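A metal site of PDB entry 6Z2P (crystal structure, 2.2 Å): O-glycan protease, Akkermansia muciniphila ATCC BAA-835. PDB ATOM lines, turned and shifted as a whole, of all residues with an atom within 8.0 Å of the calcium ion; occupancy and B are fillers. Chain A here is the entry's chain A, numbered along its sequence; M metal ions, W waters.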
ATOM      1  N   ILE A 284      24.041 -22.668  13.719  1.00  0.00           N
ATOM      2  CA  ILE A 284      25.177 -22.348  14.579  1.00  0.00           C
ATOM      3  C   ILE A 284      26.458 -22.830  13.908  1.00  0.00           C
ATOM      4  O   ILE A 284      26.626 -24.039  13.690  1.00  0.00           O
ATOM      5  CB  ILE A 284      25.010 -22.983  15.974  1.00  0.00           C
ATOM      6  CG1 ILE A 284      23.703 -22.492  16.604  1.00  0.00           C
ATOM      7  CG2 ILE A 284      26.215 -22.660  16.850  1.00  0.00           C
ATOM      8  CD1 ILE A 284      23.484 -22.921  18.030  1.00  0.00           C
ATOM      9  N   GLN A 285      27.366 -21.911  13.607  1.00  0.00           N
ATOM     10  CA  GLN A 285      28.572 -22.279  12.882  1.00  0.00           C
ATOM     11  C   GLN A 285      29.785 -21.487  13.373  1.00  0.00           C
ATOM     12  O   GLN A 285      29.677 -20.482  14.066  1.00  0.00           O
ATOM     13  CB  GLN A 285      28.403 -22.059  11.371  1.00  0.00           C
ATOM     14  CG  GLN A 285      28.083 -20.637  11.015  1.00  0.00           C
ATOM     15  CD  GLN A 285      28.113 -20.384   9.508  1.00  0.00           C
ATOM     16  OE1 GLN A 285      29.056 -20.781   8.808  1.00  0.00           O
ATOM     17  NE2 GLN A 285      27.087 -19.729   9.012  1.00  0.00           N
ATOM     18  N   ASP A 286      30.967 -21.984  12.984  1.00  0.00           N
ATOM     19  CA  ASP A 286      32.244 -21.297  13.130  1.00  0.00           C
ATOM     20  C   ASP A 286      32.458 -20.379  11.925  1.00  0.00           C
ATOM     21  O   ASP A 286      31.856 -20.575  10.870  1.00  0.00           O
ATOM     22  CB  ASP A 286      33.386 -22.310  13.194  1.00  0.00           C
ATOM     23  CG  ASP A 286      33.448 -23.063  14.515  1.00  0.00           C
ATOM     24  OD1 ASP A 286      32.835 -22.610  15.500  1.00  0.00           O
ATOM     25  OD2 ASP A 286      34.129 -24.105  14.568  1.00  0.00           O
ATOM     26  N   PRO A 287      33.315 -19.370  12.059  1.00  0.00           N
ATOM     27  CA  PRO A 287      33.740 -18.595  10.886  1.00  0.00           C
ATOM     28  C   PRO A 287      34.684 -19.394  10.025  1.00  0.00           C
ATOM     29  O   PRO A 287      35.279 -20.382  10.478  1.00  0.00           O
ATOM     30  CB  PRO A 287      34.436 -17.371  11.519  1.00  0.00           C
ATOM     31  CG  PRO A 287      34.924 -17.875  12.815  1.00  0.00           C
ATOM     32  CD  PRO A 287      33.833 -18.781  13.307  1.00  0.00           C
ATOM     33  N   PRO A 288      34.852 -19.015   8.738  1.00  0.00           N
ATOM     34  CA  PRO A 288      34.157 -17.897   8.066  1.00  0.00           C
ATOM     35  C   PRO A 288      32.697 -18.240   7.733  1.00  0.00           C
ATOM     36  O   PRO A 288      32.334 -19.430   7.756  1.00  0.00           O
ATOM     37  CB  PRO A 288      34.999 -17.659   6.815  1.00  0.00           C
ATOM     38  CG  PRO A 288      35.638 -18.994   6.539  1.00  0.00           C
ATOM     39  CD  PRO A 288      35.800 -19.697   7.841  1.00  0.00           C
ATOM     40  N   TYR A 289      31.862 -17.235   7.436  1.00  0.00           N
ATOM     41  CA  TYR A 289      30.406 -17.401   7.413  1.00  0.00           C
ATOM     42  C   TYR A 289      29.754 -17.446   6.024  1.00  0.00           C
ATOM     43  O   TYR A 289      28.534 -17.599   5.948  1.00  0.00           O
ATOM     44  CB  TYR A 289      29.752 -16.276   8.221  1.00  0.00           C
ATOM     45  CG  TYR A 289      30.226 -16.201   9.648  1.00  0.00           C
ATOM     46  CD1 TYR A 289      30.117 -17.306  10.475  1.00  0.00           C
ATOM     47  CD2 TYR A 289      30.808 -15.040  10.169  1.00  0.00           C
ATOM     48  CE1 TYR A 289      30.545 -17.266  11.794  1.00  0.00           C
ATOM     49  CE2 TYR A 289      31.265 -14.985  11.484  1.00  0.00           C
ATOM     50  CZ  TYR A 289      31.120 -16.109  12.291  1.00  0.00           C
ATOM     51  OH  TYR A 289      31.542 -16.095  13.590  1.00  0.00           O
ATOM     52  N   ALA A 290      30.510 -17.320   4.930  1.00  0.00           N
ATOM     53  CA  ALA A 290      29.863 -17.178   3.623  1.00  0.00           C
ATOM     54  C   ALA A 290      29.107 -18.451   3.222  1.00  0.00           C
ATOM     55  O   ALA A 290      29.385 -19.554   3.720  1.00  0.00           O
ATOM     56  CB  ALA A 290      30.893 -16.842   2.532  1.00  0.00           C
ATOM     57  N   VAL A 291      28.169 -18.279   2.282  1.00  0.00           N
ATOM     58  CA  VAL A 291      27.230 -19.310   1.882  1.00  0.00           C
ATOM     59  C   VAL A 291      27.908 -20.573   1.358  1.00  0.00           C
ATOM     60  O   VAL A 291      27.242 -21.610   1.250  1.00  0.00           O
ATOM     61  CB  VAL A 291      26.233 -18.790   0.817  1.00  0.00           C
ATOM     62  N   ASN A 292      29.206 -20.522   1.048  1.00  0.00           N
ATOM     63  CA  ASN A 292      29.960 -21.719   0.709  1.00  0.00           C
ATOM     64  C   ASN A 292      31.034 -22.039   1.738  1.00  0.00           C
ATOM     65  O   ASN A 292      31.959 -22.804   1.434  1.00  0.00           O
ATOM     66  CB  ASN A 292      30.571 -21.563  -0.670  1.00  0.00           C
ATOM     67  CG  ASN A 292      29.526 -21.345  -1.698  1.00  0.00           C
ATOM     68  OD1 ASN A 292      28.413 -21.847  -1.530  1.00  0.00           O
ATOM     69  ND2 ASN A 292      29.843 -20.619  -2.758  1.00  0.00           N
ATOM     70  N   GLN A 293      30.933 -21.465   2.936  1.00  0.00           N
ATOM     71  CA  GLN A 293      31.810 -21.823   4.044  1.00  0.00           C
ATOM     72  C   GLN A 293      31.021 -22.372   5.231  1.00  0.00           C
ATOM     73  O   GLN A 293      31.521 -22.358   6.357  1.00  0.00           O
ATOM     74  CB  GLN A 293      32.648 -20.606   4.485  1.00  0.00           C
ATOM     75  CG  GLN A 293      33.646 -20.078   3.444  1.00  0.00           C
ATOM     76  CD  GLN A 293      34.746 -21.089   3.116  1.00  0.00           C
ATOM     77  OE1 GLN A 293      35.117 -21.917   3.951  1.00  0.00           O
ATOM     78  NE2 GLN A 293      35.286 -21.003   1.899  1.00  0.00           N
ATOM     79  N   ASP A 294      29.795 -22.843   4.990  1.00  0.00           N
ATOM     80  CA  ASP A 294      28.826 -23.140   6.044  1.00  0.00           C
ATOM     81  C   ASP A 294      28.417 -24.609   6.069  1.00  0.00           C
ATOM     82  O   ASP A 294      27.312 -24.955   6.519  1.00  0.00           O
ATOM     83  CB  ASP A 294      27.593 -22.235   5.886  1.00  0.00           C
ATOM     84  CG  ASP A 294      26.870 -22.438   4.536  1.00  0.00           C
ATOM     85  OD1 ASP A 294      27.497 -22.949   3.576  1.00  0.00           O
ATOM     86  OD2 ASP A 294      25.679 -22.056   4.413  1.00  0.00           O
ATOM     87  N   TYR A 295      29.308 -25.513   5.623  1.00  0.00           N
ATOM     88  CA  TYR A 295      29.039 -26.967   5.653  1.00  0.00           C
ATOM     89  C   TYR A 295      29.107 -27.463   7.099  1.00  0.00           C
ATOM     90  O   TYR A 295      28.810 -28.645   7.361  1.00  0.00           O
ATOM     91  CB  TYR A 295      30.051 -27.711   4.772  1.00  0.00           C
ATOM     92  CG  TYR A 295      30.114 -27.235   3.340  1.00  0.00           C
ATOM     93  CD1 TYR A 295      29.291 -27.765   2.362  1.00  0.00           C
ATOM     94  CD2 TYR A 295      31.003 -26.233   2.969  1.00  0.00           C
ATOM     95  CE1 TYR A 295      29.356 -27.328   1.054  1.00  0.00           C
ATOM     96  CE2 TYR A 295      31.077 -25.782   1.656  1.00  0.00           C
ATOM     97  CZ  TYR A 295      30.243 -26.329   0.692  1.00  0.00           C
ATOM     98  OH  TYR A 295      30.316 -25.897  -0.596  1.00  0.00           O
ATOM     99  N   ASP A 296      29.490 -26.581   8.031  1.00  0.00           N
ATOM    100  CA  ASP A 296      29.605 -26.883   9.448  1.00  0.00           C
ATOM    101  C   ASP A 296      28.445 -26.325  10.258  1.00  0.00           C
ATOM    102  O   ASP A 296      28.462 -26.442  11.485  1.00  0.00           O
ATOM    103  CB  ASP A 296      30.911 -26.297   9.995  1.00  0.00           C
ATOM    104  CG  ASP A 296      30.896 -24.765  10.012  1.00  0.00           C
ATOM    105  OD1 ASP A 296      30.914 -24.155  11.104  1.00  0.00           O
ATOM    106  OD2 ASP A 296      30.843 -24.156   8.920  1.00  0.00           O
ATOM    107  N   ALA A 297      27.465 -25.684   9.623  1.00  0.00           N
ATOM    108  CA  ALA A 297      26.384 -25.045  10.370  1.00  0.00           C
ATOM    109  C   ALA A 297      25.446 -26.111  10.896  1.00  0.00           C
ATOM    110  O   ALA A 297      24.710 -26.729  10.128  1.00  0.00           O
ATOM    111  CB  ALA A 297      25.641 -24.055   9.485  1.00  0.00           C
ATOM    112  N   LEU A 323      32.108 -28.056  15.815  1.00  0.00           N
ATOM    113  CA  LEU A 323      32.429 -26.658  16.119  1.00  0.00           C
ATOM    114  C   LEU A 323      33.608 -26.608  17.085  1.00  0.00           C
ATOM    115  O   LEU A 323      33.571 -27.203  18.165  1.00  0.00           O
ATOM    116  CB  LEU A 323      31.218 -25.925  16.686  1.00  0.00           C
ATOM    117  CG  LEU A 323      30.029 -25.858  15.715  1.00  0.00           C
ATOM    118  CD1 LEU A 323      29.006 -24.866  16.200  1.00  0.00           C
ATOM    119  CD2 LEU A 323      30.469 -25.528  14.284  1.00  0.00           C
ATOM    120  N   ARG A 329      28.695 -18.105  15.431  1.00  0.00           N
ATOM    121  CA  ARG A 329      27.541 -17.284  15.062  1.00  0.00           C
ATOM    122  C   ARG A 329      26.252 -18.094  15.139  1.00  0.00           C
ATOM    123  O   ARG A 329      26.221 -19.268  14.770  1.00  0.00           O
ATOM    124  CB  ARG A 329      27.676 -16.719  13.643  1.00  0.00           C
ATOM    125  CG  ARG A 329      26.723 -15.548  13.380  1.00  0.00           C
ATOM    126  CD  ARG A 329      27.008 -14.848  12.057  1.00  0.00           C
ATOM    127  NE  ARG A 329      26.673 -15.733  10.948  1.00  0.00           N
ATOM    128  CZ  ARG A 329      26.566 -15.339   9.677  1.00  0.00           C
ATOM    129  NH1 ARG A 329      26.792 -14.081   9.350  1.00  0.00           N
ATOM    130  NH2 ARG A 329      26.234 -16.223   8.737  1.00  0.00           N
HETATM  131 CA    CA M   1      31.347 -21.597   8.715  1.00  0.00          CA
HETATM  132  O   HOH W   1      33.557 -22.726   8.683  1.00  0.00           O
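The backbone NH (N) of Arg 329 lies within hydrogen-bond range of the backbone carbonyl oxygen (O) of Gln 285 (2.9 Å).
OD1 of Asp 294 sits close to O of Val 291, at 2.7 Å.
Asp 294 touches the calcium ion.
Of the 16 residues printed, 6 come within 4 Å of the calcium ion.
The calcium ion is bound by OE1 of Gln 285, at 2.4 Å.
The calcium ion is bound by O of Asp 286, 2.4 Å away.
Water W1 binds the calcium ion, at 2.5 Å.
The calcium ion is bound by the backbone carbonyl oxygen (O) of Gln 293 (2.5 Å).
The backbone carbonyl oxygen (O) of Pro 288 is bound to the calcium ion, 2.6 Å away.
OD2 of Asp 296 binds the calcium ion.
The calcium ion has six donor atoms within binding distance.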
